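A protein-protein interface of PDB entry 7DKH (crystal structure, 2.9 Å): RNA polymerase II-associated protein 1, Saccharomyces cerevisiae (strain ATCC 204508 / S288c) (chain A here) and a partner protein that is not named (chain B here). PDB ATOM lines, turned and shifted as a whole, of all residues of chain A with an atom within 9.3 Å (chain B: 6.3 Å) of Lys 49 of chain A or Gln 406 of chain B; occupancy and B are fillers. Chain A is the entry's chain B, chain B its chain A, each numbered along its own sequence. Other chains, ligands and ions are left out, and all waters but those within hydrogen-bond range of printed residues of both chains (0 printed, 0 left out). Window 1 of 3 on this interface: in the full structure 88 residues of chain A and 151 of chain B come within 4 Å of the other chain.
NH2 of Arg 264 of chain B is in hydrogen-bond range of OG1 of Thr 53 of chain A (3.0 Å).
The side-chain hydroxyl of Ser 45 of chain A lies within hydrogen-bond range of the side-chain amide nitrogen of Gln 458 of chain B (3.4 Å).
The side-chain amide oxygen (OE1) of Gln 406 of chain B sits at hydrogen-bond distance from the side-chain amino group (NZ) of Lys 49 of chain A (3.3 Å).
The guanidinium group (NE) of Arg 264 of chain B sits at hydrogen-bond distance from the side-chain amide oxygen (OD1) of Asn 51 of chain A, 3.0 Å away.
The side-chain carboxylate (OE2) of Glu 407 of chain B is in salt-bridge range of the side-chain amino group (NZ) of Lys 49 of chain A (2.8 Å).
The side-chain amide oxygen of Gln 458 of chain B lies within hydrogen-bond range of the side-chain amino group of Lys 49 of chain A, 3.4 Å away.
The side-chain hydroxyl of Ser 45 of chain A is in hydrogen-bond range of the side-chain carboxylate of Glu 407 of chain B (2.8 Å).
Among the printed residues, pairs that only touch across the chains: Leu 42 of chain A with Glu 407 of chain B, Leu 42 of chain A with Tyr 410 of chain B, Leu 42 of chain A with Ile 411 of chain B, Leu 46 of chain A with Leu 405 of chain B, Leu 46 of chain A with Glu 407 of chain B, Ile 48 of chain A with Phe 267 of chain B and Asn 51 of chain A with Phe 267 of chain B.
Of the printed residues of chain B, Ile 48 of chain A touches Phe 267 (3.8 Å).
Thr 50 of chain A touches none of the printed residues of chain B.
Of the printed residues of chain B, Thr 53 of chain A touches Arg 264.
Of the printed residues of chain A, Arg 264 of chain B touches Asn 51 and Thr 53.
Printed residues of chain A within 4 Å of Phe 267 of chain B: Ile 48 and Asn 51.
Of chain A, only Lys 49 comes within 4 Å of Gln 406 of chain B.
Of chain A, only Leu 42 (3.5 Å), Ser 45 (2.8 Å), Leu 46 (3.6 Å) and Lys 49 (2.8 Å) come within 4 Å of Glu 407 of chain B.
No residue of chain A comes within 4 Å of Thr 452 of chain B.
The nearest residue of chain B that does not touch Lys 49 of chain A is Arg 264 of chain B (4.1 Å).
The side-chain hydroxyl (OG1) of Thr 53 of chain A sits at hydrogen-bond distance from the backbone carbonyl oxygen (O) of Thr 50 of chain A (3.2 Å).
The backbone carbonyl oxygen of Ile 48 of chain A sits at hydrogen-bond distance from the side-chain amide nitrogen of Asn 51 of chain A (3.5 Å).
O of Arg 264 of chain B sits at hydrogen-bond distance from OG1 of Thr 268 of chain B.
The backbone carbonyl oxygen (O) of Leu 405 of chain B is in hydrogen-bond range of the side-chain amide nitrogen (ND2) of Asn 409 of chain B, 2.6 Å away.
The backbone carbonyl oxygen of Leu 46 of chain A sits at hydrogen-bond distance from the side-chain hydroxyl of Thr 50 of chain A, at 3.3 Å.
Hydrophobic or aromatic side chains of chain B within 4 Å of the printed part of chain A: Phe 267, Leu 405, Tyr 410 and Ile 411.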
ATOM      1  N   GLN A  41       4.695 -20.236  13.417  1.00  0.00           N
ATOM      2  CA  GLN A  41       4.956 -20.275  14.844  1.00  0.00           C
ATOM      3  C   GLN A  41       3.909 -21.087  15.590  1.00  0.00           C
ATOM      4  O   GLN A  41       4.203 -21.589  16.673  1.00  0.00           O
ATOM      5  CB  GLN A  41       5.028 -18.855  15.399  1.00  0.00           C
ATOM      6  CG  GLN A  41       5.849 -17.870  14.557  1.00  0.00           C
ATOM      7  CD  GLN A  41       7.224 -18.404  14.154  1.00  0.00           C
ATOM      8  OE1 GLN A  41       7.874 -19.122  14.915  1.00  0.00           O
ATOM      9  NE2 GLN A  41       7.682 -18.025  12.966  1.00  0.00           N
ATOM     10  N   LEU A  42       2.711 -21.251  15.028  1.00  0.00           N
ATOM     11  CA  LEU A  42       1.739 -22.147  15.648  1.00  0.00           C
ATOM     12  C   LEU A  42       2.191 -23.600  15.559  1.00  0.00           C
ATOM     13  O   LEU A  42       2.119 -24.351  16.546  1.00  0.00           O
ATOM     14  CB  LEU A  42       0.370 -21.942  15.006  1.00  0.00           C
ATOM     15  CG  LEU A  42      -0.160 -20.515  15.229  1.00  0.00           C
ATOM     16  CD1 LEU A  42      -1.370 -20.186  14.365  1.00  0.00           C
ATOM     17  CD2 LEU A  42      -0.481 -20.302  16.702  1.00  0.00           C
ATOM     18  N   ILE A  43       2.704 -24.002  14.396  1.00  0.00           N
ATOM     19  CA  ILE A  43       3.255 -25.346  14.255  1.00  0.00           C
ATOM     20  C   ILE A  43       4.449 -25.536  15.182  1.00  0.00           C
ATOM     21  O   ILE A  43       4.646 -26.614  15.752  1.00  0.00           O
ATOM     22  CB  ILE A  43       3.623 -25.625  12.786  1.00  0.00           C
ATOM     23  CG1 ILE A  43       2.377 -25.530  11.901  1.00  0.00           C
ATOM     24  CG2 ILE A  43       4.277 -26.993  12.658  1.00  0.00           C
ATOM     25  CD1 ILE A  43       2.542 -26.180  10.550  1.00  0.00           C
ATOM     26  N   ASN A  44       5.265 -24.495  15.348  1.00  0.00           N
ATOM     27  CA  ASN A  44       6.372 -24.583  16.300  1.00  0.00           C
ATOM     28  C   ASN A  44       5.878 -24.684  17.743  1.00  0.00           C
ATOM     29  O   ASN A  44       6.427 -25.455  18.540  1.00  0.00           O
ATOM     30  CB  ASN A  44       7.304 -23.384  16.127  1.00  0.00           C
ATOM     31  CG  ASN A  44       8.053 -23.432  14.822  1.00  0.00           C
ATOM     32  OD1 ASN A  44       8.200 -24.502  14.226  1.00  0.00           O
ATOM     33  ND2 ASN A  44       8.526 -22.278  14.360  1.00  0.00           N
ATOM     34  N   SER A  45       4.886 -23.865  18.106  1.00  0.00           N
ATOM     35  CA  SER A  45       4.204 -23.972  19.393  1.00  0.00           C
ATOM     36  C   SER A  45       3.827 -25.415  19.691  1.00  0.00           C
ATOM     37  O   SER A  45       4.056 -25.916  20.798  1.00  0.00           O
ATOM     38  CB  SER A  45       2.959 -23.077  19.400  1.00  0.00           C
ATOM     39  OG  SER A  45       2.103 -23.362  20.497  1.00  0.00           O
ATOM     40  N   LEU A  46       3.227 -26.089  18.705  1.00  0.00           N
ATOM     41  CA  LEU A  46       2.826 -27.483  18.884  1.00  0.00           C
ATOM     42  C   LEU A  46       4.034 -28.415  18.942  1.00  0.00           C
ATOM     43  O   LEU A  46       4.043 -29.384  19.717  1.00  0.00           O
ATOM     44  CB  LEU A  46       1.887 -27.901  17.757  1.00  0.00           C
ATOM     45  CG  LEU A  46       1.330 -29.324  17.857  1.00  0.00           C
ATOM     46  CD1 LEU A  46       0.819 -29.621  19.257  1.00  0.00           C
ATOM     47  CD2 LEU A  46       0.220 -29.542  16.849  1.00  0.00           C
ATOM     48  N   TYR A  47       5.052 -28.153  18.114  1.00  0.00           N
ATOM     49  CA  TYR A  47       6.233 -29.008  18.087  1.00  0.00           C
ATOM     50  C   TYR A  47       6.919 -29.026  19.441  1.00  0.00           C
ATOM     51  O   TYR A  47       7.482 -30.049  19.849  1.00  0.00           O
ATOM     52  CB  TYR A  47       7.220 -28.552  17.009  1.00  0.00           C
ATOM     53  CG  TYR A  47       8.453 -29.432  16.971  1.00  0.00           C
ATOM     54  CD1 TYR A  47       8.452 -30.625  16.265  1.00  0.00           C
ATOM     55  CD2 TYR A  47       9.607 -29.083  17.667  1.00  0.00           C
ATOM     56  CE1 TYR A  47       9.563 -31.436  16.240  1.00  0.00           C
ATOM     57  CE2 TYR A  47      10.724 -29.892  17.654  1.00  0.00           C
ATOM     58  CZ  TYR A  47      10.695 -31.068  16.937  1.00  0.00           C
ATOM     59  OH  TYR A  47      11.806 -31.880  16.913  1.00  0.00           O
ATOM     60  N   ILE A  48       6.919 -27.885  20.135  1.00  0.00           N
ATOM     61  CA  ILE A  48       7.519 -27.831  21.468  1.00  0.00           C
ATOM     62  C   ILE A  48       6.938 -28.928  22.353  1.00  0.00           C
ATOM     63  O   ILE A  48       7.655 -29.552  23.144  1.00  0.00           O
ATOM     64  CB  ILE A  48       7.324 -26.435  22.093  1.00  0.00           C
ATOM     65  CG1 ILE A  48       8.192 -25.405  21.369  1.00  0.00           C
ATOM     66  CG2 ILE A  48       7.584 -26.462  23.605  1.00  0.00           C
ATOM     67  CD1 ILE A  48       8.109 -24.034  21.973  1.00  0.00           C
ATOM     68  N   LYS A  49       5.647 -29.228  22.181  1.00  0.00           N
ATOM     69  CA  LYS A  49       5.000 -30.270  22.976  1.00  0.00           C
ATOM     70  C   LYS A  49       5.190 -31.671  22.395  1.00  0.00           C
ATOM     71  O   LYS A  49       5.537 -32.600  23.133  1.00  0.00           O
ATOM     72  CB  LYS A  49       3.511 -29.958  23.123  1.00  0.00           C
ATOM     73  CG  LYS A  49       3.223 -28.884  24.151  1.00  0.00           C
ATOM     74  CD  LYS A  49       1.774 -28.451  24.125  1.00  0.00           C
ATOM     75  CE  LYS A  49       1.579 -27.318  23.132  1.00  0.00           C
ATOM     76  NZ  LYS A  49       0.189 -26.771  23.172  1.00  0.00           N
ATOM     77  N   THR A  50       4.980 -31.853  21.088  1.00  0.00           N
ATOM     78  CA  THR A  50       4.927 -33.183  20.477  1.00  0.00           C
ATOM     79  C   THR A  50       6.245 -33.626  19.823  1.00  0.00           C
ATOM     80  O   THR A  50       6.225 -34.499  18.949  1.00  0.00           O
ATOM     81  CB  THR A  50       3.806 -33.248  19.437  1.00  0.00           C
ATOM     82  OG1 THR A  50       4.143 -32.405  18.332  1.00  0.00           O
ATOM     83  CG2 THR A  50       2.516 -32.765  20.022  1.00  0.00           C
ATOM     84  N   ASN A  51       7.381 -33.062  20.240  1.00  0.00           N
ATOM     85  CA  ASN A  51       8.617 -32.969  19.452  1.00  0.00           C
ATOM     86  C   ASN A  51       9.041 -34.177  18.608  1.00  0.00           C
ATOM     87  O   ASN A  51       8.995 -34.101  17.377  1.00  0.00           O
ATOM     88  CB  ASN A  51       9.761 -32.612  20.410  1.00  0.00           C
ATOM     89  CG  ASN A  51       9.665 -33.362  21.739  1.00  0.00           C
ATOM     90  OD1 ASN A  51       9.983 -34.556  21.822  1.00  0.00           O
ATOM     91  ND2 ASN A  51       9.197 -32.664  22.779  1.00  0.00           N
ATOM     92  N   VAL A  52       9.436 -35.294  19.218  1.00  0.00           N
ATOM     93  CA  VAL A  52      10.064 -36.382  18.474  1.00  0.00           C
ATOM     94  C   VAL A  52       9.231 -37.660  18.545  1.00  0.00           C
ATOM     95  O   VAL A  52       9.762 -38.761  18.402  1.00  0.00           O
ATOM     96  CB  VAL A  52      11.507 -36.625  18.957  1.00  0.00           C
ATOM     97  CG1 VAL A  52      12.366 -35.410  18.677  1.00  0.00           C
ATOM     98  CG2 VAL A  52      11.519 -36.933  20.441  1.00  0.00           C
ATOM     99  N   THR A  53       7.921 -37.514  18.775  1.00  0.00           N
ATOM    100  CA  THR A  53       7.070 -38.657  19.095  1.00  0.00           C
ATOM    101  C   THR A  53       7.022 -39.692  17.973  1.00  0.00           C
ATOM    102  O   THR A  53       6.965 -40.899  18.242  1.00  0.00           O
ATOM    103  CB  THR A  53       5.662 -38.153  19.418  1.00  0.00           C
ATOM    104  OG1 THR A  53       5.751 -37.209  20.486  1.00  0.00           O
ATOM    105  CG2 THR A  53       4.764 -39.294  19.846  1.00  0.00           C
ATOM    106  N   ARG B 264      13.634 -34.455  23.670  1.00  0.00           N
ATOM    107  CA  ARG B 264      12.345 -34.211  24.318  1.00  0.00           C
ATOM    108  C   ARG B 264      12.514 -33.563  25.696  1.00  0.00           C
ATOM    109  O   ARG B 264      11.708 -32.702  26.088  1.00  0.00           O
ATOM    110  CB  ARG B 264      11.558 -35.527  24.389  1.00  0.00           C
ATOM    111  CG  ARG B 264      10.654 -35.711  25.585  1.00  0.00           C
ATOM    112  CD  ARG B 264       9.336 -34.961  25.449  1.00  0.00           C
ATOM    113  NE  ARG B 264       8.538 -35.323  24.285  1.00  0.00           N
ATOM    114  CZ  ARG B 264       7.552 -36.218  24.298  1.00  0.00           C
ATOM    115  NH1 ARG B 264       7.275 -36.894  25.407  1.00  0.00           N
ATOM    116  NH2 ARG B 264       6.860 -36.466  23.190  1.00  0.00           N
ATOM    117  N   PHE B 267      13.132 -29.767  26.065  1.00  0.00           N
ATOM    118  CA  PHE B 267      11.893 -29.009  26.146  1.00  0.00           C
ATOM    119  C   PHE B 267      11.187 -29.204  27.486  1.00  0.00           C
ATOM    120  O   PHE B 267      10.730 -28.229  28.090  1.00  0.00           O
ATOM    121  CB  PHE B 267      10.952 -29.402  25.002  1.00  0.00           C
ATOM    122  CG  PHE B 267      11.475 -29.057  23.632  1.00  0.00           C
ATOM    123  CD1 PHE B 267      11.654 -27.735  23.246  1.00  0.00           C
ATOM    124  CD2 PHE B 267      11.757 -30.058  22.716  1.00  0.00           C
ATOM    125  CE1 PHE B 267      12.133 -27.425  21.973  1.00  0.00           C
ATOM    126  CE2 PHE B 267      12.231 -29.754  21.449  1.00  0.00           C
ATOM    127  CZ  PHE B 267      12.418 -28.436  21.076  1.00  0.00           C
ATOM    128  N   THR B 268      11.067 -30.448  27.957  1.00  0.00           N
ATOM    129  CA  THR B 268      10.268 -30.681  29.159  1.00  0.00           C
ATOM    130  C   THR B 268      10.985 -30.300  30.455  1.00  0.00           C
ATOM    131  O   THR B 268      10.318 -29.956  31.437  1.00  0.00           O
ATOM    132  CB  THR B 268       9.833 -32.147  29.221  1.00  0.00           C
ATOM    133  OG1 THR B 268      10.988 -32.991  29.261  1.00  0.00           O
ATOM    134  CG2 THR B 268       9.019 -32.502  28.001  1.00  0.00           C
ATOM    135  N   ASN B 402      -9.253 -34.047  17.172  1.00  0.00           N
ATOM    136  CA  ASN B 402      -8.248 -33.308  17.938  1.00  0.00           C
ATOM    137  C   ASN B 402      -8.835 -32.048  18.557  1.00  0.00           C
ATOM    138  O   ASN B 402      -8.175 -31.006  18.626  1.00  0.00           O
ATOM    139  CB  ASN B 402      -7.039 -32.958  17.075  1.00  0.00           C
ATOM    140  CG  ASN B 402      -6.236 -34.172  16.704  1.00  0.00           C
ATOM    141  OD1 ASN B 402      -5.308 -34.559  17.417  1.00  0.00           O
ATOM    142  ND2 ASN B 402      -6.596 -34.799  15.590  1.00  0.00           N
ATOM    143  N   GLU B 403     -10.087 -32.126  19.016  1.00  0.00           N
ATOM    144  CA  GLU B 403     -10.786 -30.950  19.532  1.00  0.00           C
ATOM    145  C   GLU B 403     -10.104 -30.316  20.743  1.00  0.00           C
ATOM    146  O   GLU B 403     -10.423 -29.172  21.083  1.00  0.00           O
ATOM    147  CB  GLU B 403     -12.226 -31.304  19.917  1.00  0.00           C
ATOM    148  CG  GLU B 403     -12.340 -32.438  20.936  1.00  0.00           C
ATOM    149  CD  GLU B 403     -12.175 -33.819  20.326  1.00  0.00           C
ATOM    150  OE1 GLU B 403     -13.010 -34.193  19.476  1.00  0.00           O
ATOM    151  OE2 GLU B 403     -11.210 -34.526  20.685  1.00  0.00           O
ATOM    152  N   SER B 404      -9.187 -31.020  21.408  1.00  0.00           N
ATOM    153  CA  SER B 404      -8.507 -30.478  22.580  1.00  0.00           C
ATOM    154  C   SER B 404      -7.143 -29.882  22.256  1.00  0.00           C
ATOM    155  O   SER B 404      -6.374 -29.582  23.174  1.00  0.00           O
ATOM    156  CB  SER B 404      -8.347 -31.564  23.647  1.00  0.00           C
ATOM    157  OG  SER B 404      -7.932 -32.793  23.078  1.00  0.00           O
ATOM    158  N   LEU B 405      -6.838 -29.677  20.979  1.00  0.00           N
ATOM    159  CA  LEU B 405      -5.561 -29.109  20.557  1.00  0.00           C
ATOM    160  C   LEU B 405      -5.659 -27.583  20.556  1.00  0.00           C
ATOM    161  O   LEU B 405      -6.481 -27.015  19.830  1.00  0.00           O
ATOM    162  CB  LEU B 405      -5.205 -29.665  19.176  1.00  0.00           C
ATOM    163  CG  LEU B 405      -3.788 -29.600  18.610  1.00  0.00           C
ATOM    164  CD1 LEU B 405      -2.805 -30.148  19.614  1.00  0.00           C
ATOM    165  CD2 LEU B 405      -3.741 -30.426  17.338  1.00  0.00           C
ATOM    166  N   GLN B 406      -4.835 -26.919  21.378  1.00  0.00           N
ATOM    167  CA  GLN B 406      -4.915 -25.460  21.487  1.00  0.00           C
ATOM    168  C   GLN B 406      -4.668 -24.795  20.144  1.00  0.00           C
ATOM    169  O   GLN B 406      -5.421 -23.902  19.727  1.00  0.00           O
ATOM    170  CB  GLN B 406      -3.911 -24.915  22.506  1.00  0.00           C
ATOM    171  CG  GLN B 406      -3.594 -25.769  23.708  1.00  0.00           C
ATOM    172  CD  GLN B 406      -2.485 -25.136  24.531  1.00  0.00           C
ATOM    173  OE1 GLN B 406      -1.793 -24.231  24.061  1.00  0.00           O
ATOM    174  NE2 GLN B 406      -2.340 -25.576  25.776  1.00  0.00           N
ATOM    175  N   GLU B 407      -3.591 -25.201  19.467  1.00  0.00           N
ATOM    176  CA  GLU B 407      -3.232 -24.557  18.210  1.00  0.00           C
ATOM    177  C   GLU B 407      -4.354 -24.685  17.176  1.00  0.00           C
ATOM    178  O   GLU B 407      -4.618 -23.745  16.411  1.00  0.00           O
ATOM    179  CB  GLU B 407      -1.933 -25.157  17.673  1.00  0.00           C
ATOM    180  CG  GLU B 407      -0.692 -24.900  18.540  1.00  0.00           C
ATOM    181  CD  GLU B 407      -0.681 -25.701  19.835  1.00  0.00           C
ATOM    182  OE1 GLU B 407      -1.607 -26.514  20.040  1.00  0.00           O
ATOM    183  OE2 GLU B 407       0.253 -25.517  20.649  1.00  0.00           O
ATOM    184  N   LEU B 408      -5.057 -25.819  17.164  1.00  0.00           N
ATOM    185  CA  LEU B 408      -6.131 -25.995  16.191  1.00  0.00           C
ATOM    186  C   LEU B 408      -7.345 -25.131  16.534  1.00  0.00           C
ATOM    187  O   LEU B 408      -7.977 -24.555  15.642  1.00  0.00           O
ATOM    188  CB  LEU B 408      -6.494 -27.475  16.101  1.00  0.00           C
ATOM    189  CG  LEU B 408      -7.550 -27.876  15.075  1.00  0.00           C
ATOM    190  CD1 LEU B 408      -7.116 -27.338  13.754  1.00  0.00           C
ATOM    191  CD2 LEU B 408      -7.709 -29.388  15.019  1.00  0.00           C
ATOM    192  N   ASN B 409      -7.681 -25.024  17.819  1.00  0.00           N
ATOM    193  CA  ASN B 409      -8.769 -24.141  18.219  1.00  0.00           C
ATOM    194  C   ASN B 409      -8.431 -22.692  17.895  1.00  0.00           C
ATOM    195  O   ASN B 409      -9.281 -21.948  17.395  1.00  0.00           O
ATOM    196  CB  ASN B 409      -9.056 -24.313  19.713  1.00  0.00           C
ATOM    197  CG  ASN B 409      -9.796 -25.604  20.028  1.00  0.00           C
ATOM    198  OD1 ASN B 409     -11.006 -25.601  20.214  1.00  0.00           O
ATOM    199  ND2 ASN B 409      -9.070 -26.711  20.094  1.00  0.00           N
ATOM    200  N   TYR B 410      -7.172 -22.293  18.111  1.00  0.00           N
ATOM    201  CA  TYR B 410      -6.743 -20.941  17.755  1.00  0.00           C
ATOM    202  C   TYR B 410      -6.903 -20.689  16.260  1.00  0.00           C
ATOM    203  O   TYR B 410      -7.457 -19.662  15.844  1.00  0.00           O
ATOM    204  CB  TYR B 410      -5.290 -20.715  18.178  1.00  0.00           C
ATOM    205  CG  TYR B 410      -4.766 -19.331  17.846  1.00  0.00           C
ATOM    206  CD1 TYR B 410      -4.200 -19.057  16.602  1.00  0.00           C
ATOM    207  CD2 TYR B 410      -4.823 -18.299  18.776  1.00  0.00           C
ATOM    208  CE1 TYR B 410      -3.725 -17.785  16.290  1.00  0.00           C
ATOM    209  CE2 TYR B 410      -4.339 -17.022  18.465  1.00  0.00           C
ATOM    210  CZ  TYR B 410      -3.794 -16.778  17.225  1.00  0.00           C
ATOM    211  OH  TYR B 410      -3.313 -15.523  16.910  1.00  0.00           O
ATOM    212  N   ILE B 411      -6.389 -21.604  15.434  1.00  0.00           N
ATOM    213  CA  ILE B 411      -6.428 -21.425  13.984  1.00  0.00           C
ATOM    214  C   ILE B 411      -7.866 -21.344  13.485  1.00  0.00           C
ATOM    215  O   ILE B 411      -8.212 -20.468  12.682  1.00  0.00           O
ATOM    216  CB  ILE B 411      -5.648 -22.555  13.287  1.00  0.00           C
ATOM    217  CG1 ILE B 411      -4.153 -22.277  13.390  1.00  0.00           C
ATOM    218  CG2 ILE B 411      -6.052 -22.699  11.820  1.00  0.00           C
ATOM    219  CD1 ILE B 411      -3.292 -23.398  12.920  1.00  0.00           C
ATOM    220  N   ARG B 447     -12.461 -21.835  23.516  1.00  0.00           N
ATOM    221  CA  ARG B 447     -11.904 -23.148  23.824  1.00  0.00           C
ATOM    222  C   ARG B 447     -10.375 -23.110  23.806  1.00  0.00           C
ATOM    223  O   ARG B 447      -9.717 -23.761  24.633  1.00  0.00           O
ATOM    224  CB  ARG B 447     -12.423 -24.184  22.830  1.00  0.00           C
ATOM    225  CG  ARG B 447     -12.334 -25.582  23.359  1.00  0.00           C
ATOM    226  CD  ARG B 447     -13.708 -26.070  23.782  1.00  0.00           C
ATOM    227  NE  ARG B 447     -13.620 -27.104  24.808  1.00  0.00           N
ATOM    228  CZ  ARG B 447     -13.162 -28.337  24.618  1.00  0.00           C
ATOM    229  NH1 ARG B 447     -12.746 -28.722  23.419  1.00  0.00           N
ATOM    230  NH2 ARG B 447     -13.124 -29.187  25.636  1.00  0.00           N
ATOM    231  N   TYR B 448      -9.795 -22.323  22.892  1.00  0.00           N
ATOM    232  CA  TYR B 448      -8.352 -22.090  22.927  1.00  0.00           C
ATOM    233  C   TYR B 448      -7.930 -21.515  24.270  1.00  0.00           C
ATOM    234  O   TYR B 448      -6.967 -21.979  24.891  1.00  0.00           O
ATOM    235  CB  TYR B 448      -7.925 -21.140  21.806  1.00  0.00           C
ATOM    236  CG  TYR B 448      -6.559 -20.531  22.051  1.00  0.00           C
ATOM    237  CD1 TYR B 448      -5.393 -21.265  21.776  1.00  0.00           C
ATOM    238  CD2 TYR B 448      -6.431 -19.231  22.570  1.00  0.00           C
ATOM    239  CE1 TYR B 448      -4.135 -20.731  22.004  1.00  0.00           C
ATOM    240  CE2 TYR B 448      -5.178 -18.676  22.809  1.00  0.00           C
ATOM    241  CZ  TYR B 448      -4.034 -19.437  22.517  1.00  0.00           C
ATOM    242  OH  TYR B 448      -2.791 -18.901  22.750  1.00  0.00           O
ATOM    243  N   LEU B 451      -8.179 -24.046  27.128  1.00  0.00           N
ATOM    244  CA  LEU B 451      -7.161 -25.090  27.079  1.00  0.00           C
ATOM    245  C   LEU B 451      -5.778 -24.548  27.424  1.00  0.00           C
ATOM    246  O   LEU B 451      -4.997 -25.220  28.113  1.00  0.00           O
ATOM    247  CB  LEU B 451      -7.146 -25.732  25.692  1.00  0.00           C
ATOM    248  CG  LEU B 451      -8.319 -26.607  25.255  1.00  0.00           C
ATOM    249  CD1 LEU B 451      -8.445 -26.602  23.736  1.00  0.00           C
ATOM    250  CD2 LEU B 451      -8.096 -28.011  25.763  1.00  0.00           C
ATOM    251  N   THR B 452      -5.459 -23.336  26.965  1.00  0.00           N
ATOM    252  CA  THR B 452      -4.142 -22.768  27.229  1.00  0.00           C
ATOM    253  C   THR B 452      -3.946 -22.452  28.708  1.00  0.00           C
ATOM    254  O   THR B 452      -2.857 -22.668  29.255  1.00  0.00           O
ATOM    255  CB  THR B 452      -3.939 -21.509  26.396  1.00  0.00           C
ATOM    256  OG1 THR B 452      -4.383 -21.740  25.056  1.00  0.00           O
ATOM    257  CG2 THR B 452      -2.472 -21.155  26.355  1.00  0.00           C
ATOM    258  N   LEU B 453      -4.980 -21.929  29.368  1.00  0.00           N
ATOM    259  CA  LEU B 453      -4.875 -21.601  30.783  1.00  0.00           C
ATOM    260  C   LEU B 453      -4.944 -22.824  31.687  1.00  0.00           C
ATOM    261  O   LEU B 453      -4.488 -22.748  32.832  1.00  0.00           O
ATOM    262  CB  LEU B 453      -5.968 -20.599  31.163  1.00  0.00           C
ATOM    263  CG  LEU B 453      -5.796 -19.205  30.550  1.00  0.00           C
ATOM    264  CD1 LEU B 453      -7.005 -18.317  30.798  1.00  0.00           C
ATOM    265  CD2 LEU B 453      -4.530 -18.549  31.087  1.00  0.00           C
ATOM    266  N   THR B 455      -3.199 -25.564  31.169  1.00  0.00           N
ATOM    267  CA  THR B 455      -1.758 -25.704  31.319  1.00  0.00           C
ATOM    268  C   THR B 455      -1.137 -24.401  31.812  1.00  0.00           C
ATOM    269  O   THR B 455      -1.643 -23.308  31.548  1.00  0.00           O
ATOM    270  CB  THR B 455      -1.121 -26.116  29.990  1.00  0.00           C
ATOM    271  OG1 THR B 455      -0.795 -24.944  29.232  1.00  0.00           O
ATOM    272  CG2 THR B 455      -2.072 -26.992  29.181  1.00  0.00           C
ATOM    273  N   ASN B 457       2.447 -23.938  31.476  1.00  0.00           N
ATOM    274  CA  ASN B 457       3.784 -23.806  30.913  1.00  0.00           C
ATOM    275  C   ASN B 457       3.855 -22.804  29.770  1.00  0.00           C
ATOM    276  O   ASN B 457       4.907 -22.188  29.569  1.00  0.00           O
ATOM    277  CB  ASN B 457       4.309 -25.165  30.436  1.00  0.00           C
ATOM    278  CG  ASN B 457       3.509 -25.735  29.281  1.00  0.00           C
ATOM    279  OD1 ASN B 457       2.362 -25.350  29.050  1.00  0.00           O
ATOM    280  ND2 ASN B 457       4.117 -26.660  28.545  1.00  0.00           N
ATOM    281  N   GLN B 458       2.772 -22.628  29.018  1.00  0.00           N
ATOM    282  CA  GLN B 458       2.761 -21.784  27.834  1.00  0.00           C
ATOM    283  C   GLN B 458       1.872 -20.570  28.066  1.00  0.00           C
ATOM    284  O   GLN B 458       0.878 -20.638  28.795  1.00  0.00           O
ATOM    285  CB  GLN B 458       2.288 -22.568  26.605  1.00  0.00           C
ATOM    286  CG  GLN B 458       2.961 -22.167  25.296  1.00  0.00           C
ATOM    287  CD  GLN B 458       2.837 -23.245  24.236  1.00  0.00           C
ATOM    288  OE1 GLN B 458       1.853 -23.984  24.200  1.00  0.00           O
ATOM    289  NE2 GLN B 458       3.850 -23.359  23.382  1.00  0.00           N
ATOM    290  N   LEU B 459       2.240 -19.458  27.439  1.00  0.00           N
ATOM    291  CA  LEU B 459       1.488 -18.218  27.554  1.00  0.00           C
ATOM    292  C   LEU B 459       0.423 -18.116  26.470  1.00  0.00           C
ATOM    293  O   LEU B 459       0.439 -18.837  25.468  1.00  0.00           O
ATOM    294  CB  LEU B 459       2.406 -16.997  27.437  1.00  0.00           C
ATOM    295  CG  LEU B 459       3.257 -16.457  28.587  1.00  0.00           C
ATOM    296  CD1 LEU B 459       4.477 -15.731  28.029  1.00  0.00           C
ATOM    297  CD2 LEU B 459       2.448 -15.526  29.477  1.00  0.00           C
